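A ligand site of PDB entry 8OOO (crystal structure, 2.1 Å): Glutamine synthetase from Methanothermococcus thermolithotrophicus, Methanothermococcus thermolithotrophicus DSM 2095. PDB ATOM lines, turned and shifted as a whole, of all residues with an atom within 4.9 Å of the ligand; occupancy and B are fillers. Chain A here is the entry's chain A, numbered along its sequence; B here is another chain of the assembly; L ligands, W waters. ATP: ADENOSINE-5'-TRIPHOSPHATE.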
ATOM      1  N   PHE A 133     -10.687  -9.016 -19.313  1.00  0.00           N
ATOM      2  CA  PHE A 133     -11.380  -9.436 -18.109  1.00  0.00           C
ATOM      3  C   PHE A 133     -12.663  -8.659 -17.941  1.00  0.00           C
ATOM      4  O   PHE A 133     -12.647  -7.431 -18.019  1.00  0.00           O
ATOM      5  CB  PHE A 133     -10.468  -9.238 -16.881  1.00  0.00           C
ATOM      6  CG  PHE A 133      -9.356 -10.260 -16.841  1.00  0.00           C
ATOM      7  CD1 PHE A 133      -9.621 -11.568 -16.492  1.00  0.00           C
ATOM      8  CD2 PHE A 133      -8.079  -9.940 -17.294  1.00  0.00           C
ATOM      9  CE1 PHE A 133      -8.638 -12.527 -16.574  1.00  0.00           C
ATOM     10  CE2 PHE A 133      -7.088 -10.916 -17.353  1.00  0.00           C
ATOM     11  CZ  PHE A 133      -7.386 -12.208 -17.024  1.00  0.00           C
ATOM     12  N   VAL A 134     -13.767  -9.365 -17.662  1.00  0.00           N
ATOM     13  CA  VAL A 134     -15.066  -8.758 -17.486  1.00  0.00           C
ATOM     14  C   VAL A 134     -15.723  -9.255 -16.204  1.00  0.00           C
ATOM     15  O   VAL A 134     -15.678 -10.443 -15.941  1.00  0.00           O
ATOM     16  CB  VAL A 134     -16.003  -9.039 -18.719  1.00  0.00           C
ATOM     17  CG1 VAL A 134     -17.374  -8.368 -18.533  1.00  0.00           C
ATOM     18  CG2 VAL A 134     -15.339  -8.551 -20.017  1.00  0.00           C
ATOM     19  N   GLY A 135     -16.326  -8.325 -15.457  1.00  0.00           N
ATOM     20  CA  GLY A 135     -17.109  -8.576 -14.256  1.00  0.00           C
ATOM     21  C   GLY A 135     -18.497  -7.986 -14.420  1.00  0.00           C
ATOM     22  O   GLY A 135     -18.663  -6.785 -14.226  1.00  0.00           O
ATOM     23  N   PRO A 136     -19.501  -8.780 -14.870  1.00  0.00           N
ATOM     24  CA  PRO A 136     -20.839  -8.229 -15.124  1.00  0.00           C
ATOM     25  C   PRO A 136     -21.752  -8.397 -13.925  1.00  0.00           C
ATOM     26  O   PRO A 136     -21.575  -9.343 -13.142  1.00  0.00           O
ATOM     27  CB  PRO A 136     -21.333  -9.097 -16.292  1.00  0.00           C
ATOM     28  CG  PRO A 136     -20.772 -10.445 -15.982  1.00  0.00           C
ATOM     29  CD  PRO A 136     -19.464 -10.213 -15.192  1.00  0.00           C
ATOM     30  N   GLU A 137     -22.768  -7.521 -13.791  1.00  0.00           N
ATOM     31  CA  GLU A 137     -23.669  -7.531 -12.643  1.00  0.00           C
ATOM     32  C   GLU A 137     -25.094  -7.612 -13.128  1.00  0.00           C
ATOM     33  O   GLU A 137     -25.803  -6.602 -13.112  1.00  0.00           O
ATOM     34  CB  GLU A 137     -23.444  -6.277 -11.796  1.00  0.00           C
ATOM     35  CG  GLU A 137     -21.981  -6.011 -11.485  1.00  0.00           C
ATOM     36  CD  GLU A 137     -21.766  -4.805 -10.594  1.00  0.00           C
ATOM     37  OE1 GLU A 137     -22.029  -3.652 -11.002  1.00  0.00           O
ATOM     38  OE2 GLU A 137     -21.323  -5.028  -9.445  1.00  0.00           O
ATOM     39  N   GLU A 189     -19.386 -13.153  -4.803  1.00  0.00           N
ATOM     40  CA  GLU A 189     -18.808 -12.062  -4.037  1.00  0.00           C
ATOM     41  C   GLU A 189     -19.770 -11.444  -3.030  1.00  0.00           C
ATOM     42  O   GLU A 189     -19.338 -10.997  -1.974  1.00  0.00           O
ATOM     43  CB  GLU A 189     -18.315 -10.960  -4.988  1.00  0.00           C
ATOM     44  CG  GLU A 189     -17.097 -11.350  -5.801  1.00  0.00           C
ATOM     45  CD  GLU A 189     -16.570 -10.237  -6.683  1.00  0.00           C
ATOM     46  OE1 GLU A 189     -17.318  -9.253  -6.886  1.00  0.00           O
ATOM     47  OE2 GLU A 189     -15.412 -10.342  -7.162  1.00  0.00           O
ATOM     48  N   GLU A 201     -29.544  -8.659  -6.500  1.00  0.00           N
ATOM     49  CA  GLU A 201     -28.253  -8.717  -7.150  1.00  0.00           C
ATOM     50  C   GLU A 201     -27.406  -9.773  -6.462  1.00  0.00           C
ATOM     51  O   GLU A 201     -27.408  -9.873  -5.226  1.00  0.00           O
ATOM     52  CB  GLU A 201     -27.552  -7.353  -7.082  1.00  0.00           C
ATOM     53  CG  GLU A 201     -26.334  -7.301  -7.986  1.00  0.00           C
ATOM     54  CD  GLU A 201     -25.698  -5.943  -8.169  1.00  0.00           C
ATOM     55  OE1 GLU A 201     -26.415  -4.922  -8.067  1.00  0.00           O
ATOM     56  OE2 GLU A 201     -24.480  -5.916  -8.426  1.00  0.00           O
ATOM     57  N   ASP A 203     -23.501 -10.921  -7.029  1.00  0.00           N
ATOM     58  CA  ASP A 203     -22.258 -10.643  -7.739  1.00  0.00           C
ATOM     59  C   ASP A 203     -21.312 -11.817  -7.704  1.00  0.00           C
ATOM     60  O   ASP A 203     -21.262 -12.560  -6.706  1.00  0.00           O
ATOM     61  CB  ASP A 203     -21.579  -9.424  -7.139  1.00  0.00           C
ATOM     62  CG  ASP A 203     -22.348  -8.138  -7.337  1.00  0.00           C
ATOM     63  OD1 ASP A 203     -23.178  -8.074  -8.269  1.00  0.00           O
ATOM     64  OD2 ASP A 203     -22.125  -7.177  -6.558  1.00  0.00           O
ATOM     65  N   PHE A 204     -20.576 -12.028  -8.797  1.00  0.00           N
ATOM     66  CA  PHE A 204     -19.601 -13.112  -8.891  1.00  0.00           C
ATOM     67  C   PHE A 204     -18.300 -12.518  -9.436  1.00  0.00           C
ATOM     68  O   PHE A 204     -18.292 -11.412 -10.007  1.00  0.00           O
ATOM     69  CB  PHE A 204     -20.135 -14.286  -9.752  1.00  0.00           C
ATOM     70  CG  PHE A 204     -20.659 -13.945 -11.139  1.00  0.00           C
ATOM     71  CD1 PHE A 204     -21.978 -13.595 -11.331  1.00  0.00           C
ATOM     72  CD2 PHE A 204     -19.829 -14.019 -12.250  1.00  0.00           C
ATOM     73  CE1 PHE A 204     -22.459 -13.335 -12.612  1.00  0.00           C
ATOM     74  CE2 PHE A 204     -20.322 -13.753 -13.526  1.00  0.00           C
ATOM     75  CZ  PHE A 204     -21.646 -13.440 -13.702  1.00  0.00           C
ATOM     76  N   LYS A 205     -17.197 -13.182  -9.151  1.00  0.00           N
ATOM     77  CA  LYS A 205     -15.892 -12.648  -9.509  1.00  0.00           C
ATOM     78  C   LYS A 205     -15.686 -12.581 -11.038  1.00  0.00           C
ATOM     79  O   LYS A 205     -16.089 -13.482 -11.779  1.00  0.00           O
ATOM     80  CB  LYS A 205     -14.777 -13.476  -8.872  1.00  0.00           C
ATOM     81  CG  LYS A 205     -13.441 -12.796  -8.968  1.00  0.00           C
ATOM     82  CD  LYS A 205     -12.355 -13.649  -8.438  1.00  0.00           C
ATOM     83  CE  LYS A 205     -10.986 -13.009  -8.548  1.00  0.00           C
ATOM     84  NZ  LYS A 205      -9.937 -13.836  -7.915  1.00  0.00           N
ATOM     85  N   PHE A 206     -14.987 -11.542 -11.488  1.00  0.00           N
ATOM     86  CA  PHE A 206     -14.667 -11.360 -12.883  1.00  0.00           C
ATOM     87  C   PHE A 206     -13.730 -12.469 -13.351  1.00  0.00           C
ATOM     88  O   PHE A 206     -13.093 -13.125 -12.523  1.00  0.00           O
ATOM     89  CB  PHE A 206     -13.989 -10.009 -13.105  1.00  0.00           C
ATOM     90  CG  PHE A 206     -12.586  -9.944 -12.561  1.00  0.00           C
ATOM     91  CD1 PHE A 206     -12.360  -9.680 -11.223  1.00  0.00           C
ATOM     92  CD2 PHE A 206     -11.495 -10.173 -13.376  1.00  0.00           C
ATOM     93  CE1 PHE A 206     -11.057  -9.591 -10.721  1.00  0.00           C
ATOM     94  CE2 PHE A 206     -10.205 -10.133 -12.867  1.00  0.00           C
ATOM     95  CZ  PHE A 206      -9.989  -9.806 -11.553  1.00  0.00           C
ATOM     96  N   HIS A 250     -24.206  -3.894 -15.614  1.00  0.00           N
ATOM     97  CA  HIS A 250     -22.983  -3.092 -15.712  1.00  0.00           C
ATOM     98  C   HIS A 250     -21.808  -4.051 -15.941  1.00  0.00           C
ATOM     99  O   HIS A 250     -21.773  -5.114 -15.326  1.00  0.00           O
ATOM    100  CB  HIS A 250     -22.730  -2.320 -14.405  1.00  0.00           C
ATOM    101  CG  HIS A 250     -23.870  -1.444 -13.987  1.00  0.00           C
ATOM    102  ND1 HIS A 250     -24.012  -1.039 -12.683  1.00  0.00           N
ATOM    103  CD2 HIS A 250     -24.905  -0.947 -14.710  1.00  0.00           C
ATOM    104  CE1 HIS A 250     -25.108  -0.299 -12.645  1.00  0.00           C
ATOM    105  NE2 HIS A 250     -25.668  -0.218 -13.844  1.00  0.00           N
ATOM    106  N   HIS A 252     -17.926  -4.367 -15.659  1.00  0.00           N
ATOM    107  CA  HIS A 252     -16.623  -3.901 -15.206  1.00  0.00           C
ATOM    108  C   HIS A 252     -15.637  -4.624 -16.101  1.00  0.00           C
ATOM    109  O   HIS A 252     -15.785  -5.829 -16.330  1.00  0.00           O
ATOM    110  CB  HIS A 252     -16.377  -4.262 -13.734  1.00  0.00           C
ATOM    111  CG  HIS A 252     -17.254  -3.518 -12.755  1.00  0.00           C
ATOM    112  ND1 HIS A 252     -16.720  -2.670 -11.824  1.00  0.00           N
ATOM    113  CD2 HIS A 252     -18.601  -3.543 -12.601  1.00  0.00           C
ATOM    114  CE1 HIS A 252     -17.748  -2.169 -11.132  1.00  0.00           C
ATOM    115  NE2 HIS A 252     -18.899  -2.675 -11.562  1.00  0.00           N
ATOM    116  N   GLN A 253     -14.674  -3.915 -16.656  1.00  0.00           N
ATOM    117  CA  GLN A 253     -13.757  -4.543 -17.581  1.00  0.00           C
ATOM    118  C   GLN A 253     -12.398  -3.903 -17.539  1.00  0.00           C
ATOM    119  O   GLN A 253     -12.249  -2.724 -17.189  1.00  0.00           O
ATOM    120  CB  GLN A 253     -14.343  -4.513 -18.991  1.00  0.00           C
ATOM    121  CG  GLN A 253     -14.595  -3.100 -19.516  1.00  0.00           C
ATOM    122  CD  GLN A 253     -15.631  -3.096 -20.624  1.00  0.00           C
ATOM    123  OE1 GLN A 253     -15.310  -3.171 -21.816  1.00  0.00           O
ATOM    124  NE2 GLN A 253     -16.887  -2.970 -20.257  1.00  0.00           N
ATOM    125  N   SER A 254     -11.393  -4.702 -17.885  1.00  0.00           N
ATOM    126  CA  SER A 254     -10.007  -4.264 -17.909  1.00  0.00           C
ATOM    127  C   SER A 254      -9.218  -5.150 -18.841  1.00  0.00           C
ATOM    128  O   SER A 254      -9.609  -6.276 -19.079  1.00  0.00           O
ATOM    129  CB  SER A 254      -9.402  -4.295 -16.513  1.00  0.00           C
ATOM    130  OG  SER A 254      -9.358  -5.598 -15.965  1.00  0.00           O
ATOM    131  N   TRP A 256      -5.347  -6.700 -19.566  1.00  0.00           N
ATOM    132  CA  TRP A 256      -4.064  -6.959 -18.919  1.00  0.00           C
ATOM    133  C   TRP A 256      -3.073  -7.342 -19.998  1.00  0.00           C
ATOM    134  O   TRP A 256      -3.279  -8.337 -20.692  1.00  0.00           O
ATOM    135  CB  TRP A 256      -4.215  -8.084 -17.884  1.00  0.00           C
ATOM    136  CG  TRP A 256      -5.066  -7.725 -16.688  1.00  0.00           C
ATOM    137  CD1 TRP A 256      -6.318  -7.189 -16.695  1.00  0.00           C
ATOM    138  CD2 TRP A 256      -4.726  -7.932 -15.314  1.00  0.00           C
ATOM    139  NE1 TRP A 256      -6.787  -7.051 -15.417  1.00  0.00           N
ATOM    140  CE2 TRP A 256      -5.837  -7.531 -14.547  1.00  0.00           C
ATOM    141  CE3 TRP A 256      -3.622  -8.491 -14.662  1.00  0.00           C
ATOM    142  CZ2 TRP A 256      -5.860  -7.658 -13.150  1.00  0.00           C
ATOM    143  CZ3 TRP A 256      -3.641  -8.562 -13.293  1.00  0.00           C
ATOM    144  CH2 TRP A 256      -4.738  -8.152 -12.549  1.00  0.00           C
ATOM    145  N   ARG A 321     -22.061   7.849 -10.607  1.00  0.00           N
ATOM    146  CA  ARG A 321     -22.973   6.960 -11.293  1.00  0.00           C
ATOM    147  C   ARG A 321     -23.925   7.691 -12.256  1.00  0.00           C
ATOM    148  O   ARG A 321     -24.930   7.109 -12.645  1.00  0.00           O
ATOM    149  CB  ARG A 321     -23.732   6.099 -10.264  1.00  0.00           C
ATOM    150  CG  ARG A 321     -22.811   5.189  -9.463  1.00  0.00           C
ATOM    151  CD  ARG A 321     -23.525   4.517  -8.295  1.00  0.00           C
ATOM    152  NE  ARG A 321     -22.828   3.298  -7.887  1.00  0.00           N
ATOM    153  CZ  ARG A 321     -21.710   3.259  -7.146  1.00  0.00           C
ATOM    154  NH1 ARG A 321     -21.127   2.094  -6.872  1.00  0.00           N
ATOM    155  NH2 ARG A 321     -21.178   4.377  -6.676  1.00  0.00           N
ATOM    156  N   ARG A 326     -18.385   4.696 -15.331  1.00  0.00           N
ATOM    157  CA  ARG A 326     -17.920   5.089 -14.006  1.00  0.00           C
ATOM    158  C   ARG A 326     -16.590   4.334 -13.795  1.00  0.00           C
ATOM    159  O   ARG A 326     -16.456   3.201 -14.252  1.00  0.00           O
ATOM    160  CB  ARG A 326     -18.923   4.685 -12.904  1.00  0.00           C
ATOM    161  CG  ARG A 326     -18.322   4.811 -11.483  1.00  0.00           C
ATOM    162  CD  ARG A 326     -19.327   4.462 -10.421  1.00  0.00           C
ATOM    163  NE  ARG A 326     -19.500   3.015 -10.370  1.00  0.00           N
ATOM    164  CZ  ARG A 326     -18.905   2.197  -9.501  1.00  0.00           C
ATOM    165  NH1 ARG A 326     -18.142   2.676  -8.538  1.00  0.00           N
ATOM    166  NH2 ARG A 326     -19.128   0.887  -9.564  1.00  0.00           N
ATOM    167  N   PRO A 328     -14.543   2.854 -10.854  1.00  0.00           N
ATOM    168  CA  PRO A 328     -14.622   2.670  -9.392  1.00  0.00           C
ATOM    169  C   PRO A 328     -13.367   3.176  -8.680  1.00  0.00           C
ATOM    170  O   PRO A 328     -12.287   3.260  -9.287  1.00  0.00           O
ATOM    171  CB  PRO A 328     -14.819   1.156  -9.233  1.00  0.00           C
ATOM    172  CG  PRO A 328     -15.335   0.691 -10.531  1.00  0.00           C
ATOM    173  CD  PRO A 328     -14.700   1.566 -11.559  1.00  0.00           C
ATOM    174  N   LYS A 333      -4.714  -3.976  -8.887  1.00  0.00           N
ATOM    175  CA  LYS A 333      -5.299  -5.054  -9.723  1.00  0.00           C
ATOM    176  C   LYS A 333      -6.807  -4.805  -9.835  1.00  0.00           C
ATOM    177  O   LYS A 333      -7.411  -5.362 -10.716  1.00  0.00           O
ATOM    178  CB  LYS A 333      -4.873  -6.407  -9.157  1.00  0.00           C
ATOM    179  CG  LYS A 333      -3.469  -6.832  -9.573  1.00  0.00           C
ATOM    180  CD  LYS A 333      -2.805  -7.845  -8.671  1.00  0.00           C
ATOM    181  CE  LYS A 333      -1.773  -8.671  -9.388  1.00  0.00           C
ATOM    182  NZ  LYS A 333      -2.031 -10.124  -9.285  1.00  0.00           N
ATOM    183  N   GLY A 334      -7.355  -3.949  -8.980  1.00  0.00           N
ATOM    184  CA  GLY A 334      -8.783  -3.604  -8.988  1.00  0.00           C
ATOM    185  C   GLY A 334      -9.099  -2.438  -9.904  1.00  0.00           C
ATOM    186  O   GLY A 334     -10.250  -2.075  -9.973  1.00  0.00           O
ATOM    187  N   THR A 335      -8.105  -1.931 -10.619  1.00  0.00           N
ATOM    188  CA  THR A 335      -8.305  -0.790 -11.546  1.00  0.00           C
ATOM    189  C   THR A 335      -9.109  -1.261 -12.758  1.00  0.00           C
ATOM    190  O   THR A 335      -8.649  -2.144 -13.433  1.00  0.00           O
ATOM    191  CB  THR A 335      -6.955  -0.162 -11.909  1.00  0.00           C
ATOM    192  OG1 THR A 335      -6.432   0.351 -10.693  1.00  0.00           O
ATOM    193  CG2 THR A 335      -7.065   0.974 -12.880  1.00  0.00           C
ATOM    194  N   ARG A 336     -10.276  -0.663 -13.013  1.00  0.00           N
ATOM    195  CA  ARG A 336     -11.135  -1.084 -14.142  1.00  0.00           C
ATOM    196  C   ARG A 336     -12.149   0.010 -14.452  1.00  0.00           C
ATOM    197  O   ARG A 336     -12.225   0.970 -13.715  1.00  0.00           O
ATOM    198  CB  ARG A 336     -11.838  -2.401 -13.816  1.00  0.00           C
ATOM    199  CG  ARG A 336     -13.050  -2.247 -12.930  1.00  0.00           C
ATOM    200  CD  ARG A 336     -12.858  -2.961 -11.624  1.00  0.00           C
ATOM    201  NE  ARG A 336     -13.949  -2.899 -10.676  1.00  0.00           N
ATOM    202  CZ  ARG A 336     -13.799  -2.866  -9.373  1.00  0.00           C
ATOM    203  NH1 ARG A 336     -12.596  -2.864  -8.844  1.00  0.00           N
ATOM    204  NH2 ARG A 336     -14.852  -2.821  -8.592  1.00  0.00           N
ATOM    205  N   GLU A 338     -16.340   0.687 -15.561  1.00  0.00           N
ATOM    206  CA  GLU A 338     -17.641   0.083 -15.501  1.00  0.00           C
ATOM    207  C   GLU A 338     -18.458   0.706 -16.592  1.00  0.00           C
ATOM    208  O   GLU A 338     -18.723   1.900 -16.495  1.00  0.00           O
ATOM    209  CB  GLU A 338     -18.288   0.353 -14.138  1.00  0.00           C
ATOM    210  CG  GLU A 338     -19.657  -0.243 -13.967  1.00  0.00           C
ATOM    211  CD  GLU A 338     -20.410   0.193 -12.731  1.00  0.00           C
ATOM    212  OE1 GLU A 338     -21.070  -0.658 -12.085  1.00  0.00           O
ATOM    213  OE2 GLU A 338     -20.390   1.405 -12.429  1.00  0.00           O
ATOM    214  N   ARG A 340     -21.842   1.178 -17.917  1.00  0.00           N
ATOM    215  CA  ARG A 340     -23.110   1.073 -17.222  1.00  0.00           C
ATOM    216  C   ARG A 340     -24.333   0.856 -18.104  1.00  0.00           C
ATOM    217  O   ARG A 340     -25.392   0.460 -17.593  1.00  0.00           O
ATOM    218  CB  ARG A 340     -23.322   2.301 -16.318  1.00  0.00           C
ATOM    219  CG  ARG A 340     -22.236   2.476 -15.257  1.00  0.00           C
ATOM    220  CD  ARG A 340     -22.404   3.747 -14.440  1.00  0.00           C
ATOM    221  NE  ARG A 340     -23.687   3.773 -13.710  1.00  0.00           N
ATOM    222  CZ  ARG A 340     -23.903   3.141 -12.557  1.00  0.00           C
ATOM    223  NH1 ARG A 340     -22.918   2.447 -11.971  1.00  0.00           N
ATOM    224  NH2 ARG A 340     -25.094   3.194 -11.971  1.00  0.00           N
ATOM    225  N   TYR B  56     -17.145  -1.970  -0.394  1.00  0.00           N
ATOM    226  CA  TYR B  56     -17.729  -0.777  -0.982  1.00  0.00           C
ATOM    227  C   TYR B  56     -19.186  -0.902  -1.206  1.00  0.00           C
ATOM    228  O   TYR B  56     -19.692  -2.011  -1.394  1.00  0.00           O
ATOM    229  CB  TYR B  56     -17.062  -0.479  -2.338  1.00  0.00           C
ATOM    230  CG  TYR B  56     -15.602  -0.125  -2.229  1.00  0.00           C
ATOM    231  CD1 TYR B  56     -15.202   1.198  -2.062  1.00  0.00           C
ATOM    232  CD2 TYR B  56     -14.626  -1.088  -2.431  1.00  0.00           C
ATOM    233  CE1 TYR B  56     -13.854   1.538  -2.052  1.00  0.00           C
ATOM    234  CE2 TYR B  56     -13.276  -0.755  -2.405  1.00  0.00           C
ATOM    235  CZ  TYR B  56     -12.893   0.554  -2.167  1.00  0.00           C
ATOM    236  OH  TYR B  56     -11.553   0.910  -2.156  1.00  0.00           O
HETATM  237  PG  ATP L   1     -21.639  -1.850  -8.066  1.00  0.00           P
HETATM  238  O1G ATP L   1     -21.620  -0.669  -7.137  1.00  0.00           O
HETATM  239  O2G ATP L   1     -22.389  -2.983  -7.422  1.00  0.00           O
HETATM  240  O3G ATP L   1     -22.276  -1.473  -9.375  1.00  0.00           O
HETATM  241  PB  ATP L   1     -18.930  -1.981  -7.353  1.00  0.00           P
HETATM  242  O1B ATP L   1     -18.384  -0.646  -7.767  1.00  0.00           O
HETATM  243  O2B ATP L   1     -19.387  -1.951  -5.920  1.00  0.00           O
HETATM  244  O3B ATP L   1     -20.138  -2.360  -8.326  1.00  0.00           O
HETATM  245  PA  ATP L   1     -18.036  -4.626  -7.263  1.00  0.00           P
HETATM  246  O1A ATP L   1     -19.507  -4.866  -7.088  1.00  0.00           O
HETATM  247  O2A ATP L   1     -17.273  -5.072  -6.046  1.00  0.00           O
HETATM  248  O3A ATP L   1     -17.767  -3.066  -7.500  1.00  0.00           O
HETATM  249  O5' ATP L   1     -17.504  -5.439  -8.531  1.00  0.00           O
HETATM  250  C5' ATP L   1     -18.327  -5.670  -9.657  1.00  0.00           C
HETATM  251  C4' ATP L   1     -17.626  -6.662 -10.572  1.00  0.00           C
HETATM  252  O4' ATP L   1     -16.380  -6.131 -11.037  1.00  0.00           O
HETATM  253  C3' ATP L   1     -17.307  -7.964  -9.848  1.00  0.00           C
HETATM  254  O3' ATP L   1     -17.756  -9.057 -10.643  1.00  0.00           O
HETATM  255  C2' ATP L   1     -15.795  -7.974  -9.759  1.00  0.00           C
HETATM  256  O2' ATP L   1     -15.264  -9.296  -9.799  1.00  0.00           O
HETATM  257  C1' ATP L   1     -15.431  -7.196 -11.008  1.00  0.00           C
HETATM  258  N9  ATP L   1     -14.013  -6.761 -11.005  1.00  0.00           N
HETATM  259  C8  ATP L   1     -13.270  -6.453  -9.939  1.00  0.00           C
HETATM  260  N7  ATP L   1     -12.010  -6.107 -10.305  1.00  0.00           N
HETATM  261  C5  ATP L   1     -11.944  -6.192 -11.647  1.00  0.00           C
HETATM  262  C6  ATP L   1     -10.920  -5.966 -12.685  1.00  0.00           C
HETATM  263  N6  ATP L   1      -9.663  -5.574 -12.369  1.00  0.00           N
HETATM  264  N1  ATP L   1     -11.269  -6.185 -13.966  1.00  0.00           N
HETATM  265  C2  ATP L   1     -12.502  -6.583 -14.305  1.00  0.00           C
HETATM  266  N3  ATP L   1     -13.480  -6.800 -13.420  1.00  0.00           N
HETATM  267  C4  ATP L   1     -13.268  -6.637 -12.096  1.00  0.00           C
HETATM  268  O   HOH W   1     -20.820  -9.713 -10.674  1.00  0.00           O
HETATM  269  O   HOH W   2     -24.421   1.154  -8.987  1.00  0.00           O
HETATM  270  O   HOH W   3     -23.521  -4.973  -5.485  1.00  0.00           O
HETATM  271  O   HOH W   4     -23.665  -1.924  -4.484  1.00  0.00           O
HETATM  272  O   HOH W   5      -7.311  -4.594 -13.459  1.00  0.00           O
HETATM  273  O   HOH W   6     -15.533  -6.981  -5.950  1.00  0.00           O
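An oxygen (O1B) of the ligand is in salt-bridge range of the guanidinium group (NH2) of Arg 326, at 2.5 Å.
An oxygen (O3') of the ligand is in hydrogen-bond range of the backbone carbonyl oxygen (O) of Phe 204 (2.5 Å).
A nitrogen (N6) of the ligand lies within hydrogen-bond range of the backbone carbonyl oxygen (O) of Lys 333 (2.8 Å).
NH1 of Arg 321 lies within salt-bridge range of O1G of the ligand.
OE1 of Glu 338 sits close to O3G of the ligand (3.1 Å).
OE2 of Glu 189 lies within hydrogen-bond range of O2' of the ligand (2.8 Å).
The side-chain hydroxyl of Ser 254 lies within hydrogen-bond range of a nitrogen (N1) of the ligand (2.8 Å).
An oxygen (O2') of the ligand is in hydrogen-bond range of the backbone NH of Phe 206 (2.8 Å).
The guanidinium group (NH2) of Arg 336 is in hydrogen-bond range of an oxygen (O3A) of the ligand (3.1 Å).
An oxygen (O3G) of the ligand sits close to the side-chain carboxylate of Glu 137.
O3B of the ligand lies within hydrogen-bond range of NE2 of His 252 (3.5 Å).
The guanidinium group (NE) of Arg 336 lies within hydrogen-bond range of a ring nitrogen (ND1) of His 252 (3.0 Å).
The backbone NH of Phe 133 sits at hydrogen-bond distance from the backbone carbonyl oxygen of Ser 254 (3.0 Å).
ND1 of His 250 is in hydrogen-bond range of OE1 of Glu 338 (3.0 Å).
The guanidinium group (NH1) of Arg 336 lies within hydrogen-bond range of the backbone carbonyl oxygen (O) of Gly 334 (2.7 Å).
The side-chain hydroxyl of Ser 254 sits at hydrogen-bond distance from the indole nitrogen of Trp 256 (3.0 Å).
O of Asp 203 sits at hydrogen-bond distance from N of Glu 189, at 2.7 Å.
N of Gly 135 lies within hydrogen-bond range of O of His 252, at 2.7 Å.
The backbone carbonyl oxygen (O) of His 250 is in hydrogen-bond range of the backbone NH (N) of Glu 137.
Phe 133 touches the ligand (O to C2, 3.8 Å).
Gly 135 touches the ligand.
Glu 201 touches the ligand.
OD2 of Asp 203 touches O1A of the ligand, at 3.5 Å.
Lys 205 touches the ligand.
His 250 touches the ligand (ND1 to O3G, 3.8 Å).
O of Thr 335 touches N6 of the ligand, 3.7 Å away.
Hydrophobic or aromatic side chains that line the ligand: Phe 206 and His 252.
Within 4 Å of the ligand: Phe 133, Gly 135, Glu 137, Glu 189, Glu 201, Asp 203, Phe 204, Lys 205, Phe 206, His 250, His 252, Ser 254, Arg 321, Arg 326, Lys 333, Thr 335, Arg 336 and Glu 338.
Water W6 lies within hydrogen-bond range of O2A of the ligand (2.6 Å) and OE1 of Glu 189 (3.0 Å).
Water W5 lies within hydrogen-bond range of a nitrogen (N6) of the ligand, the backbone carbonyl oxygen (O) of Thr 335, the backbone carbonyl oxygen (O) of Lys 333, the indole nitrogen (NE1) of Trp 256 and the side-chain hydroxyl (OG) of Ser 254.
Water W3 lies within hydrogen-bond range of the side-chain carboxylate of Asp 203, an oxygen (O2G) of the ligand and the side-chain carboxylate of Glu 201.
Water W1 lies within hydrogen-bond range of the backbone carbonyl oxygen (O) of Pro 136, the backbone NH (N) of Phe 204 and an oxygen (O3') of the ligand.
Water W2 lies within hydrogen-bond range of the guanidinium group of Arg 321 (2.9 Å) and an oxygen (O3G) of the ligand (3.4 Å).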
